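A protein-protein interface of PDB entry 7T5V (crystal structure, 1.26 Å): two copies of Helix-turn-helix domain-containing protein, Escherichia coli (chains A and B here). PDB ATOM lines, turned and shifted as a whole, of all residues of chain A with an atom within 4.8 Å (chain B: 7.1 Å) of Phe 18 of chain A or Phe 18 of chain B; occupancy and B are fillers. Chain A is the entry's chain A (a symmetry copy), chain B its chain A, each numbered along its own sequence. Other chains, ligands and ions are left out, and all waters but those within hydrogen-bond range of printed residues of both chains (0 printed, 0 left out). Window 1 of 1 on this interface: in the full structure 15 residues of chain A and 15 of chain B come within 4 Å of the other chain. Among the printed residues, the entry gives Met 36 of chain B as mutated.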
ATOM      1  N   LEU A  14       4.302  18.303   9.137  1.00  0.00           N
ATOM      2  CA  LEU A  14       5.558  18.341   8.400  1.00  0.00           C
ATOM      3  C   LEU A  14       5.297  18.172   6.915  1.00  0.00           C
ATOM      4  O   LEU A  14       5.916  18.843   6.089  1.00  0.00           O
ATOM      5  CB  LEU A  14       6.504  17.249   8.886  1.00  0.00           C
ATOM      6  CG  LEU A  14       7.073  17.353  10.294  1.00  0.00           C
ATOM      7  CD1 LEU A  14       7.925  16.126  10.599  1.00  0.00           C
ATOM      8  CD2 LEU A  14       7.854  18.633  10.442  1.00  0.00           C
ATOM      9  N   ASP A  15       4.359  17.288   6.573  1.00  0.00           N
ATOM     10  CA  ASP A  15       4.060  16.987   5.183  1.00  0.00           C
ATOM     11  C   ASP A  15       3.387  18.168   4.495  1.00  0.00           C
ATOM     12  O   ASP A  15       3.712  18.505   3.359  1.00  0.00           O
ATOM     13  CB  ASP A  15       3.139  15.758   5.116  1.00  0.00           C
ATOM     14  CG  ASP A  15       3.831  14.457   5.498  1.00  0.00           C
ATOM     15  OD1 ASP A  15       5.067  14.403   5.633  1.00  0.00           O
ATOM     16  OD2 ASP A  15       3.089  13.478   5.665  1.00  0.00           O
ATOM     17  N   ASP A  16       2.417  18.799   5.164  1.00  0.00           N
ATOM     18  CA  ASP A  16       1.716  19.930   4.556  1.00  0.00           C
ATOM     19  C   ASP A  16       2.650  21.128   4.375  1.00  0.00           C
ATOM     20  O   ASP A  16       2.601  21.807   3.347  1.00  0.00           O
ATOM     21  CB  ASP A  16       0.467  20.277   5.377  1.00  0.00           C
ATOM     22  CG  ASP A  16      -0.664  19.262   5.180  1.00  0.00           C
ATOM     23  OD1 ASP A  16      -0.646  18.494   4.199  1.00  0.00           O
ATOM     24  OD2 ASP A  16      -1.592  19.245   5.999  1.00  0.00           O
ATOM     25  N   ALA A  17       3.548  21.362   5.327  1.00  0.00           N
ATOM     26  CA  ALA A  17       4.535  22.426   5.162  1.00  0.00           C
ATOM     27  C   ALA A  17       5.483  22.110   4.011  1.00  0.00           C
ATOM     28  O   ALA A  17       5.764  22.967   3.183  1.00  0.00           O
ATOM     29  CB  ALA A  17       5.329  22.595   6.449  1.00  0.00           C
ATOM     30  N   PHE A  18       5.891  20.847   3.898  1.00  0.00           N
ATOM     31  CA  PHE A  18       6.725  20.420   2.785  1.00  0.00           C
ATOM     32  C   PHE A  18       6.052  20.729   1.455  1.00  0.00           C
ATOM     33  O   PHE A  18       6.680  21.265   0.539  1.00  0.00           O
ATOM     34  CB  PHE A  18       7.010  18.924   2.909  1.00  0.00           C
ATOM     35  CG  PHE A  18       7.588  18.308   1.656  1.00  0.00           C
ATOM     36  CD1 PHE A  18       8.906  18.550   1.301  1.00  0.00           C
ATOM     37  CD2 PHE A  18       6.801  17.542   0.828  1.00  0.00           C
ATOM     38  CE1 PHE A  18       9.447  17.991   0.138  1.00  0.00           C
ATOM     39  CE2 PHE A  18       7.341  16.963  -0.323  1.00  0.00           C
ATOM     40  CZ  PHE A  18       8.639  17.216  -0.679  1.00  0.00           C
ATOM     41  N   PHE A  19       4.766  20.382   1.314  1.00  0.00           N
ATOM     42  CA  PHE A  19       4.084  20.613   0.033  1.00  0.00           C
ATOM     43  C   PHE A  19       4.025  22.096  -0.305  1.00  0.00           C
ATOM     44  O   PHE A  19       4.244  22.498  -1.457  1.00  0.00           O
ATOM     45  CB  PHE A  19       2.691  19.973   0.006  1.00  0.00           C
ATOM     46  CG  PHE A  19       2.039  19.960  -1.346  1.00  0.00           C
ATOM     47  CD1 PHE A  19       2.744  19.609  -2.472  1.00  0.00           C
ATOM     48  CD2 PHE A  19       0.690  20.246  -1.476  1.00  0.00           C
ATOM     49  CE1 PHE A  19       2.141  19.584  -3.693  1.00  0.00           C
ATOM     50  CE2 PHE A  19       0.079  20.207  -2.699  1.00  0.00           C
ATOM     51  CZ  PHE A  19       0.797  19.873  -3.809  1.00  0.00           C
ATOM     52  N   ARG A  20       3.703  22.920   0.687  1.00  0.00           N
ATOM     53  CA  ARG A  20       3.710  24.366   0.470  1.00  0.00           C
ATOM     54  C   ARG A  20       5.094  24.866   0.057  1.00  0.00           C
ATOM     55  O   ARG A  20       5.215  25.693  -0.861  1.00  0.00           O
ATOM     56  CB  ARG A  20       3.195  25.059   1.747  1.00  0.00           C
ATOM     57  CG  ARG A  20       3.329  26.595   1.792  1.00  0.00           C
ATOM     58  CD  ARG A  20       1.988  27.355   1.821  1.00  0.00           C
ATOM     59  NE  ARG A  20       1.900  28.366   2.882  1.00  0.00           N
ATOM     60  CZ  ARG A  20       2.632  29.476   2.948  1.00  0.00           C
ATOM     61  NH1 ARG A  20       3.613  29.722   2.081  1.00  0.00           N
ATOM     62  NH2 ARG A  20       2.377  30.364   3.904  1.00  0.00           N
ATOM     63  N   GLY A  21       6.149  24.386   0.709  1.00  0.00           N
ATOM     64  CA  GLY A  21       7.496  24.769   0.300  1.00  0.00           C
ATOM     65  C   GLY A  21       7.833  24.320  -1.109  1.00  0.00           C
ATOM     66  O   GLY A  21       8.434  25.061  -1.882  1.00  0.00           O
ATOM     67  N   TYR A  22       7.450  23.095  -1.455  1.00  0.00           N
ATOM     68  CA  TYR A  22       7.676  22.571  -2.799  1.00  0.00           C
ATOM     69  C   TYR A  22       6.996  23.442  -3.844  1.00  0.00           C
ATOM     70  O   TYR A  22       7.604  23.788  -4.860  1.00  0.00           O
ATOM     71  CB  TYR A  22       7.220  21.102  -2.859  1.00  0.00           C
ATOM     72  CG  TYR A  22       6.883  20.606  -4.247  1.00  0.00           C
ATOM     73  CD1 TYR A  22       5.597  20.716  -4.753  1.00  0.00           C
ATOM     74  CD2 TYR A  22       7.836  20.007  -5.036  1.00  0.00           C
ATOM     75  CE1 TYR A  22       5.289  20.284  -6.008  1.00  0.00           C
ATOM     76  CE2 TYR A  22       7.546  19.569  -6.293  1.00  0.00           C
ATOM     77  CZ  TYR A  22       6.271  19.703  -6.778  1.00  0.00           C
ATOM     78  OH  TYR A  22       6.018  19.260  -8.049  1.00  0.00           O
ATOM     79  N   LEU A  33      12.645  17.473  -7.449  1.00  0.00           N
ATOM     80  CA  LEU A  33      11.994  16.752  -6.364  1.00  0.00           C
ATOM     81  C   LEU A  33      11.118  15.626  -6.895  1.00  0.00           C
ATOM     82  O   LEU A  33      11.087  14.521  -6.333  1.00  0.00           O
ATOM     83  CB  LEU A  33      11.191  17.714  -5.484  1.00  0.00           C
ATOM     84  CG  LEU A  33      11.963  18.259  -4.288  1.00  0.00           C
ATOM     85  CD1 LEU A  33      13.086  19.096  -4.729  1.00  0.00           C
ATOM     86  CD2 LEU A  33      11.132  19.065  -3.394  1.00  0.00           C
ATOM     87  N   ARG A  34      10.425  15.860  -7.993  1.00  0.00           N
ATOM     88  CA  ARG A  34       9.626  14.794  -8.592  1.00  0.00           C
ATOM     89  C   ARG A  34      10.519  13.658  -9.090  1.00  0.00           C
ATOM     90  O   ARG A  34      10.189  12.479  -8.939  1.00  0.00           O
ATOM     91  CB  ARG A  34       8.768  15.369  -9.716  1.00  0.00           C
ATOM     92  CG  ARG A  34       7.688  16.364  -9.233  1.00  0.00           C
ATOM     93  CD  ARG A  34       6.580  16.585 -10.243  1.00  0.00           C
ATOM     94  NE  ARG A  34       7.058  17.098 -11.522  1.00  0.00           N
ATOM     95  CZ  ARG A  34       7.314  18.373 -11.771  1.00  0.00           C
ATOM     96  NH1 ARG A  34       7.217  19.311 -10.842  1.00  0.00           N
ATOM     97  NH2 ARG A  34       7.724  18.701 -12.987  1.00  0.00           N
ATOM     98  N   LEU A  37      11.523  11.547  -6.086  1.00  0.00           N
ATOM     99  CA  LEU A  37      10.434  10.653  -5.716  1.00  0.00           C
ATOM    100  C   LEU A  37      10.435   9.404  -6.592  1.00  0.00           C
ATOM    101  O   LEU A  37      10.298   8.281  -6.104  1.00  0.00           O
ATOM    102  CB  LEU A  37       9.104  11.388  -5.803  1.00  0.00           C
ATOM    103  CG  LEU A  37       7.858  10.486  -5.717  1.00  0.00           C
ATOM    104  CD1 LEU A  37       7.805   9.795  -4.403  1.00  0.00           C
ATOM    105  CD2 LEU A  37       6.552  11.257  -5.935  1.00  0.00           C
ATOM    106  N   ARG B  12      -0.541  21.945 -11.871  1.00  0.00           N
ATOM    107  CA  ARG B  12      -1.220  21.568 -10.630  1.00  0.00           C
ATOM    108  C   ARG B  12      -1.397  20.059 -10.515  1.00  0.00           C
ATOM    109  O   ARG B  12      -1.233  19.489  -9.428  1.00  0.00           O
ATOM    110  CB  ARG B  12      -2.576  22.277 -10.557  1.00  0.00           C
ATOM    111  CG  ARG B  12      -3.256  22.214  -9.184  1.00  0.00           C
ATOM    112  CD  ARG B  12      -4.643  22.897  -9.172  1.00  0.00           C
ATOM    113  NE  ARG B  12      -5.535  22.351 -10.195  1.00  0.00           N
ATOM    114  CZ  ARG B  12      -6.078  21.138 -10.151  1.00  0.00           C
ATOM    115  NH1 ARG B  12      -5.882  20.328  -9.124  1.00  0.00           N
ATOM    116  NH2 ARG B  12      -6.833  20.724 -11.167  1.00  0.00           N
ATOM    117  N   HIS B  13      -1.740  19.391 -11.613  1.00  0.00           N
ATOM    118  CA  HIS B  13      -1.924  17.947 -11.565  1.00  0.00           C
ATOM    119  C   HIS B  13      -0.610  17.224 -11.315  1.00  0.00           C
ATOM    120  O   HIS B  13      -0.577  16.242 -10.573  1.00  0.00           O
ATOM    121  CB  HIS B  13      -2.611  17.513 -12.850  1.00  0.00           C
ATOM    122  CG  HIS B  13      -4.090  17.783 -12.861  1.00  0.00           C
ATOM    123  ND1 HIS B  13      -4.730  18.446 -13.892  1.00  0.00           N
ATOM    124  CD2 HIS B  13      -5.069  17.413 -11.997  1.00  0.00           C
ATOM    125  CE1 HIS B  13      -6.027  18.498 -13.649  1.00  0.00           C
ATOM    126  NE2 HIS B  13      -6.264  17.870 -12.506  1.00  0.00           N
ATOM    127  N   LEU B  14       0.498  17.721 -11.868  1.00  0.00           N
ATOM    128  CA  LEU B  14       1.776  17.087 -11.572  1.00  0.00           C
ATOM    129  C   LEU B  14       2.108  17.239 -10.100  1.00  0.00           C
ATOM    130  O   LEU B  14       2.603  16.306  -9.469  1.00  0.00           O
ATOM    131  CB  LEU B  14       2.889  17.694 -12.419  1.00  0.00           C
ATOM    132  CG  LEU B  14       2.870  17.460 -13.922  1.00  0.00           C
ATOM    133  CD1 LEU B  14       4.021  18.215 -14.577  1.00  0.00           C
ATOM    134  CD2 LEU B  14       2.926  15.983 -14.216  1.00  0.00           C
ATOM    135  N   ASP B  15       1.810  18.414  -9.542  1.00  0.00           N
ATOM    136  CA  ASP B  15       2.137  18.709  -8.157  1.00  0.00           C
ATOM    137  C   ASP B  15       1.279  17.888  -7.202  1.00  0.00           C
ATOM    138  O   ASP B  15       1.772  17.359  -6.208  1.00  0.00           O
ATOM    139  CB  ASP B  15       1.915  20.206  -7.891  1.00  0.00           C
ATOM    140  CG  ASP B  15       2.939  21.103  -8.572  1.00  0.00           C
ATOM    141  OD1 ASP B  15       3.960  20.626  -9.101  1.00  0.00           O
ATOM    142  OD2 ASP B  15       2.686  22.317  -8.566  1.00  0.00           O
ATOM    143  N   ASP B  16      -0.026  17.793  -7.474  1.00  0.00           N
ATOM    144  CA  ASP B  16      -0.912  17.035  -6.589  1.00  0.00           C
ATOM    145  C   ASP B  16      -0.586  15.541  -6.627  1.00  0.00           C
ATOM    146  O   ASP B  16      -0.591  14.874  -5.590  1.00  0.00           O
ATOM    147  CB  ASP B  16      -2.376  17.327  -6.936  1.00  0.00           C
ATOM    148  CG  ASP B  16      -2.826  18.713  -6.463  1.00  0.00           C
ATOM    149  OD1 ASP B  16      -2.162  19.321  -5.601  1.00  0.00           O
ATOM    150  OD2 ASP B  16      -3.863  19.193  -6.939  1.00  0.00           O
ATOM    151  N   ALA B  17      -0.238  15.013  -7.797  1.00  0.00           N
ATOM    152  CA  ALA B  17       0.185  13.617  -7.878  1.00  0.00           C
ATOM    153  C   ALA B  17       1.490  13.403  -7.121  1.00  0.00           C
ATOM    154  O   ALA B  17       1.622  12.449  -6.365  1.00  0.00           O
ATOM    155  CB  ALA B  17       0.366  13.218  -9.335  1.00  0.00           C
ATOM    156  N   PHE B  18       2.417  14.351  -7.241  1.00  0.00           N
ATOM    157  CA  PHE B  18       3.663  14.289  -6.491  1.00  0.00           C
ATOM    158  C   PHE B  18       3.390  14.202  -4.996  1.00  0.00           C
ATOM    159  O   PHE B  18       3.981  13.379  -4.292  1.00  0.00           O
ATOM    160  CB  PHE B  18       4.511  15.518  -6.813  1.00  0.00           C
ATOM    161  CG  PHE B  18       5.667  15.725  -5.862  1.00  0.00           C
ATOM    162  CD1 PHE B  18       6.787  14.910  -5.933  1.00  0.00           C
ATOM    163  CD2 PHE B  18       5.603  16.692  -4.886  1.00  0.00           C
ATOM    164  CE1 PHE B  18       7.858  15.089  -5.051  1.00  0.00           C
ATOM    165  CE2 PHE B  18       6.680  16.891  -4.017  1.00  0.00           C
ATOM    166  CZ  PHE B  18       7.777  16.074  -4.079  1.00  0.00           C
ATOM    167  N   PHE B  19       2.503  15.061  -4.475  1.00  0.00           N
ATOM    168  CA  PHE B  19       2.240  15.052  -3.030  1.00  0.00           C
ATOM    169  C   PHE B  19       1.656  13.721  -2.579  1.00  0.00           C
ATOM    170  O   PHE B  19       2.036  13.178  -1.532  1.00  0.00           O
ATOM    171  CB  PHE B  19       1.354  16.229  -2.604  1.00  0.00           C
ATOM    172  CG  PHE B  19       1.246  16.421  -1.120  1.00  0.00           C
ATOM    173  CD1 PHE B  19       2.353  16.345  -0.310  1.00  0.00           C
ATOM    174  CD2 PHE B  19       0.027  16.740  -0.541  1.00  0.00           C
ATOM    175  CE1 PHE B  19       2.249  16.537   1.034  1.00  0.00           C
ATOM    176  CE2 PHE B  19      -0.077  16.946   0.806  1.00  0.00           C
ATOM    177  CZ  PHE B  19       1.030  16.851   1.598  1.00  0.00           C
ATOM    178  N   ARG B  20       0.709  13.195  -3.349  1.00  0.00           N
ATOM    179  CA  ARG B  20       0.157  11.878  -3.037  1.00  0.00           C
ATOM    180  C   ARG B  20       1.239  10.797  -3.055  1.00  0.00           C
ATOM    181  O   ARG B  20       1.277   9.933  -2.165  1.00  0.00           O
ATOM    182  CB  ARG B  20      -0.987  11.575  -4.024  1.00  0.00           C
ATOM    183  CG  ARG B  20      -1.555  10.141  -3.994  1.00  0.00           C
ATOM    184  CD  ARG B  20      -3.022  10.042  -3.533  1.00  0.00           C
ATOM    185  NE  ARG B  20      -3.876   9.253  -4.430  1.00  0.00           N
ATOM    186  CZ  ARG B  20      -3.762   7.944  -4.643  1.00  0.00           C
ATOM    187  NH1 ARG B  20      -2.764   7.233  -4.122  1.00  0.00           N
ATOM    188  NH2 ARG B  20      -4.670   7.330  -5.396  1.00  0.00           N
ATOM    189  N   GLY B  21       2.125  10.821  -4.046  1.00  0.00           N
ATOM    190  CA  GLY B  21       3.225   9.861  -4.063  1.00  0.00           C
ATOM    191  C   GLY B  21       4.156  10.012  -2.877  1.00  0.00           C
ATOM    192  O   GLY B  21       4.589   9.027  -2.284  1.00  0.00           O
ATOM    193  N   TYR B  22       4.476  11.252  -2.519  1.00  0.00           N
ATOM    194  CA  TYR B  22       5.326  11.522  -1.363  1.00  0.00           C
ATOM    195  C   TYR B  22       4.712  10.956  -0.093  1.00  0.00           C
ATOM    196  O   TYR B  22       5.400  10.305   0.698  1.00  0.00           O
ATOM    197  CB  TYR B  22       5.598  13.034  -1.271  1.00  0.00           C
ATOM    198  CG  TYR B  22       5.976  13.521   0.110  1.00  0.00           C
ATOM    199  CD1 TYR B  22       5.008  13.942   1.010  1.00  0.00           C
ATOM    200  CD2 TYR B  22       7.291  13.586   0.503  1.00  0.00           C
ATOM    201  CE1 TYR B  22       5.340  14.368   2.260  1.00  0.00           C
ATOM    202  CE2 TYR B  22       7.642  14.010   1.749  1.00  0.00           C
ATOM    203  CZ  TYR B  22       6.666  14.405   2.628  1.00  0.00           C
ATOM    204  OH  TYR B  22       7.053  14.817   3.875  1.00  0.00           O
ATOM    205  N   LYS B  23       3.394  11.118   0.074  1.00  0.00           N
ATOM    206  CA  LYS B  23       2.733  10.612   1.268  1.00  0.00           C
ATOM    207  C   LYS B  23       2.683   9.096   1.317  1.00  0.00           C
ATOM    208  O   LYS B  23       2.528   8.540   2.406  1.00  0.00           O
ATOM    209  CB  LYS B  23       1.328  11.204   1.383  1.00  0.00           C
ATOM    210  CG  LYS B  23       1.343  12.653   1.819  1.00  0.00           C
ATOM    211  CD  LYS B  23      -0.024  13.189   2.151  1.00  0.00           C
ATOM    212  CE  LYS B  23      -0.803  13.413   0.911  1.00  0.00           C
ATOM    213  NZ  LYS B  23      -2.006  14.226   1.197  1.00  0.00           N
ATOM    214  N   ASN B  24       2.836   8.423   0.180  1.00  0.00           N
ATOM    215  CA  ASN B  24       2.895   6.972   0.134  1.00  0.00           C
ATOM    216  C   ASN B  24       4.292   6.412   0.374  1.00  0.00           C
ATOM    217  O   ASN B  24       4.445   5.197   0.478  1.00  0.00           O
ATOM    218  CB  ASN B  24       2.388   6.475  -1.223  1.00  0.00           C
ATOM    219  CG  ASN B  24       0.897   6.647  -1.387  1.00  0.00           C
ATOM    220  OD1 ASN B  24       0.172   6.793  -0.409  1.00  0.00           O
ATOM    221  ND2 ASN B  24       0.431   6.643  -2.632  1.00  0.00           N
ATOM    222  N   LEU B  25       5.309   7.252   0.473  1.00  0.00           N
ATOM    223  CA  LEU B  25       6.654   6.772   0.730  1.00  0.00           C
ATOM    224  C   LEU B  25       6.798   6.378   2.195  1.00  0.00           C
ATOM    225  O   LEU B  25       6.055   6.834   3.063  1.00  0.00           O
ATOM    226  CB  LEU B  25       7.683   7.864   0.423  1.00  0.00           C
ATOM    227  CG  LEU B  25       7.920   8.281  -1.025  1.00  0.00           C
ATOM    228  CD1 LEU B  25       8.896   9.466  -1.102  1.00  0.00           C
ATOM    229  CD2 LEU B  25       8.436   7.082  -1.827  1.00  0.00           C
ATOM    230  N   LYS B  30      10.415   9.987   2.873  1.00  0.00           N
ATOM    231  CA  LYS B  30       9.821  11.315   3.003  1.00  0.00           C
ATOM    232  C   LYS B  30      10.789  12.305   3.617  1.00  0.00           C
ATOM    233  O   LYS B  30      10.939  13.426   3.114  1.00  0.00           O
ATOM    234  CB  LYS B  30       8.549  11.223   3.855  1.00  0.00           C
ATOM    235  CG  LYS B  30       7.424  10.382   3.213  1.00  0.00           C
ATOM    236  CD  LYS B  30       6.264  10.104   4.163  1.00  0.00           C
ATOM    237  CE  LYS B  30       5.518  11.360   4.466  1.00  0.00           C
ATOM    238  NZ  LYS B  30       4.488  11.120   5.517  1.00  0.00           N
ATOM    239  N   GLN B  32      14.010  12.329   3.436  1.00  0.00           N
ATOM    240  CA  GLN B  32      15.016  12.699   2.443  1.00  0.00           C
ATOM    241  C   GLN B  32      14.487  13.707   1.434  1.00  0.00           C
ATOM    242  O   GLN B  32      15.222  14.615   1.026  1.00  0.00           O
ATOM    243  CB  GLN B  32      15.571  11.467   1.739  1.00  0.00           C
ATOM    244  CG  GLN B  32      16.499  10.612   2.604  1.00  0.00           C
ATOM    245  CD  GLN B  32      17.643  11.377   3.207  1.00  0.00           C
ATOM    246  OE1 GLN B  32      18.350  12.105   2.532  1.00  0.00           O
ATOM    247  NE2 GLN B  32      17.803  11.238   4.488  1.00  0.00           N
ATOM    248  N   LEU B  33      13.214  13.593   1.042  1.00  0.00           N
ATOM    249  CA  LEU B  33      12.629  14.605   0.173  1.00  0.00           C
ATOM    250  C   LEU B  33      12.552  15.956   0.870  1.00  0.00           C
ATOM    251  O   LEU B  33      12.823  17.004   0.266  1.00  0.00           O
ATOM    252  CB  LEU B  33      11.254  14.156  -0.326  1.00  0.00           C
ATOM    253  CG  LEU B  33      11.283  13.423  -1.663  1.00  0.00           C
ATOM    254  CD1 LEU B  33      12.007  12.151  -1.544  1.00  0.00           C
ATOM    255  CD2 LEU B  33       9.946  13.127  -2.178  1.00  0.00           C
ATOM    256  N   ARG B  34      12.219  15.963   2.147  1.00  0.00           N
ATOM    257  CA  ARG B  34      12.201  17.221   2.889  1.00  0.00           C
ATOM    258  C   ARG B  34      13.606  17.817   2.986  1.00  0.00           C
ATOM    259  O   ARG B  34      13.792  19.029   2.861  1.00  0.00           O
ATOM    260  CB  ARG B  34      11.591  16.992   4.269  1.00  0.00           C
ATOM    261  CG  ARG B  34      10.096  16.603   4.236  1.00  0.00           C
ATOM    262  CD  ARG B  34       9.392  16.810   5.562  1.00  0.00           C
ATOM    263  NE  ARG B  34       9.983  16.044   6.654  1.00  0.00           N
ATOM    264  CZ  ARG B  34       9.726  14.769   6.904  1.00  0.00           C
ATOM    265  NH1 ARG B  34       8.939  14.039   6.130  1.00  0.00           N
ATOM    266  NH2 ARG B  34      10.320  14.205   7.945  1.00  0.00           N
ATOM    267  N   LYS B  35      14.621  16.973   3.159  1.00  0.00           N
ATOM    268  CA  LYS B  35      15.995  17.460   3.174  1.00  0.00           C
ATOM    269  C   LYS B  35      16.393  18.063   1.829  1.00  0.00           C
ATOM    270  O   LYS B  35      17.055  19.109   1.794  1.00  0.00           O
ATOM    271  CB  LYS B  35      16.920  16.314   3.544  1.00  0.00           C
ATOM    272  CG  LYS B  35      18.352  16.733   3.741  1.00  0.00           C
ATOM    273  CD  LYS B  35      19.218  15.529   4.034  1.00  0.00           C
ATOM    274  CE  LYS B  35      20.586  15.646   3.366  1.00  0.00           C
ATOM    275  NZ  LYS B  35      21.670  15.930   4.337  1.00  0.00           N
ATOM    276  N   MET B  36      16.002  17.436   0.718  1.00  0.00           N
ATOM    277  CA  MET B  36      16.289  17.988  -0.607  1.00  0.00           C
ATOM    278  C   MET B  36      15.643  19.365  -0.773  1.00  0.00           C
ATOM    279  O   MET B  36      16.257  20.284  -1.328  1.00  0.00           O
ATOM    280  CB  MET B  36      15.781  16.998  -1.659  1.00  0.00           C
ATOM    281  CG  MET B  36      16.143  17.358  -3.071  1.00  0.00           C
ATOM    282  SD  MET B  36      15.411  16.210  -4.238  1.00  0.00           S
ATOM    283  CE  MET B  36      16.252  16.599  -5.721  1.00  0.00           C
ATOM    284  N   LEU B  37      14.401  19.504  -0.332  1.00  0.00           N
ATOM    285  CA  LEU B  37      13.752  20.808  -0.399  1.00  0.00           C
ATOM    286  C   LEU B  37      14.576  21.862   0.333  1.00  0.00           C
ATOM    287  O   LEU B  37      14.791  22.967  -0.169  1.00  0.00           O
ATOM    288  CB  LEU B  37      12.343  20.717   0.166  1.00  0.00           C
ATOM    289  CG  LEU B  37      11.657  22.074   0.418  1.00  0.00           C
ATOM    290  CD1 LEU B  37      11.489  22.817  -0.858  1.00  0.00           C
ATOM    291  CD2 LEU B  37      10.293  21.931   1.102  1.00  0.00           C
ATOM    292  N   ASP B  38      15.041  21.529   1.532  1.00  0.00           N
ATOM    293  CA  ASP B  38      15.838  22.481   2.297  1.00  0.00           C
ATOM    294  C   ASP B  38      17.120  22.847   1.565  1.00  0.00           C
ATOM    295  O   ASP B  38      17.549  23.999   1.600  1.00  0.00           O
ATOM    296  CB  ASP B  38      16.132  21.908   3.679  1.00  0.00           C
ATOM    297  CG  ASP B  38      16.632  22.966   4.640  1.00  0.00           C
ATOM    298  OD1 ASP B  38      15.867  23.921   4.914  1.00  0.00           O
ATOM    299  OD2 ASP B  38      17.785  22.850   5.106  1.00  0.00           O
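Among the printed residues, pairs that only touch across the chains: Phe 19 of chain A with Asp 15 of chain B, Asp 15 of chain A with Phe 19 of chain B, Tyr 22 of chain A with Phe 18 of chain B, Phe 18 of chain A with Tyr 22 of chain B, Leu 37 of chain A with Leu 25 of chain B, Phe 19 of chain A with Asp 16 of chain B, Asp 16 of chain A with Phe 19 of chain B, Phe 18 of chain A with Leu 33 of chain B, Leu 33 of chain A with Phe 18 of chain B, Phe 19 of chain A with Phe 19 of chain B, Phe 18 of chain A with Leu 37 of chain B, Leu 37 of chain A with Phe 18 of chain B, Phe 18 of chain A with Phe 18 of chain B, Arg 34 of chain A with Phe 18 of chain B, Phe 18 of chain A with Arg 34 of chain B, Leu 33 of chain A with Met 36 of chain B, Gly 21 of chain A with Leu 37 of chain B, Leu 37 of chain A with Gly 21 of chain B, Tyr 22 of chain A with Leu 37 of chain B and Leu 37 of chain A with Tyr 22 of chain B.
Printed residues of chain B within 4 Å of Tyr 22 of chain A: Asp 15, Phe 18 and Leu 37.
Of the printed residues of chain B, Leu 33 of chain A touches Phe 18 and Met 36.
His 13 of chain B touches none of the printed residues of chain A.
Printed residues of chain A within 4 Å of Phe 19 of chain B: Asp 15 (3.4 Å), Asp 16 (3.5 Å) and Phe 19 (3.6 Å).
The nearest residue of chain B that does not touch Phe 18 of chain A is Phe 19 of chain B (4.7 Å).
Printed residues of chain A that touch a printed residue of chain B: Asp 15, Asp 16, Phe 18, Phe 19, Gly 21, Tyr 22, Leu 33, Arg 34 and Leu 37.
Printed residues of chain B that touch a printed residue of chain A: Asp 15, Asp 16, Phe 18, Phe 19, Gly 21, Tyr 22, Leu 25, Lys 30, Leu 33, Arg 34, Met 36 and Leu 37.
Hydrophobic or aromatic side chains of chain B that line the printed part of chain A: Phe 18, Phe 19, Tyr 22, Leu 25, Met 36 and Leu 37.
Among the printed residues, Asp or Glu carboxylates within 4 Å of a Lys or Arg side-chain nitrogen of the other chain: Asp 15 of chain A with Lys 30 of chain B, Asp 15 of chain A with Arg 34 of chain B and Arg 34 of chain A with Asp 15 of chain B.
Asp 16 of chain A touches Phe 19 of chain B, and with the chains exchanged Phe 19 of chain A touches Asp 16 of chain B.
Phe 18 of chain A touches Tyr 22 of chain B, and with the chains exchanged Tyr 22 of chain A touches Phe 18 of chain B.
Phe 19 of chain B touches its own counterpart, Phe 19 of chain A.
Gly 21 of chain A touches Leu 37 of chain B, and with the chains exchanged Leu 37 of chain A touches Gly 21 of chain B.
Positions printed for both chains: 14, 15, 16, 17, 18, 19, 20, 21, 22, 33, 34 and 37.
The guanidinium group (NH1) of Arg 34 of chain B is in salt-bridge range of the side-chain carboxylate (OD1) of Asp 15 of chain A, at 3.9 Å.
The side-chain carboxylate (OD1) of Asp 15 of chain B lies within hydrogen-bond range of the side-chain hydroxyl (OH) of Tyr 22 of chain A, 2.7 Å away.
The side-chain hydroxyl (OH) of Tyr 22 of chain B sits at hydrogen-bond distance from the side-chain carboxylate (OD1) of Asp 15 of chain A (2.7 Å).
OD1 of Asp 15 of chain B lies within salt-bridge range of NH1 of Arg 34 of chain A (3.9 Å).
The side-chain amino group (NZ) of Lys 30 of chain B is in salt-bridge range of the side-chain carboxylate (OD2) of Asp 15 of chain A (2.7 Å).
The guanidinium group (NH1) of Arg 34 of chain B lies within hydrogen-bond range of the side-chain hydroxyl (OH) of Tyr 22 of chain B (3.0 Å).
OH of Tyr 22 of chain A lies within hydrogen-bond range of NH1 of Arg 34 of chain A (3.0 Å).
The guanidinium group (NH1) of Arg 12 of chain B is in salt-bridge range of the side-chain carboxylate (OD2) of Asp 16 of chain B, 3.2 Å away.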
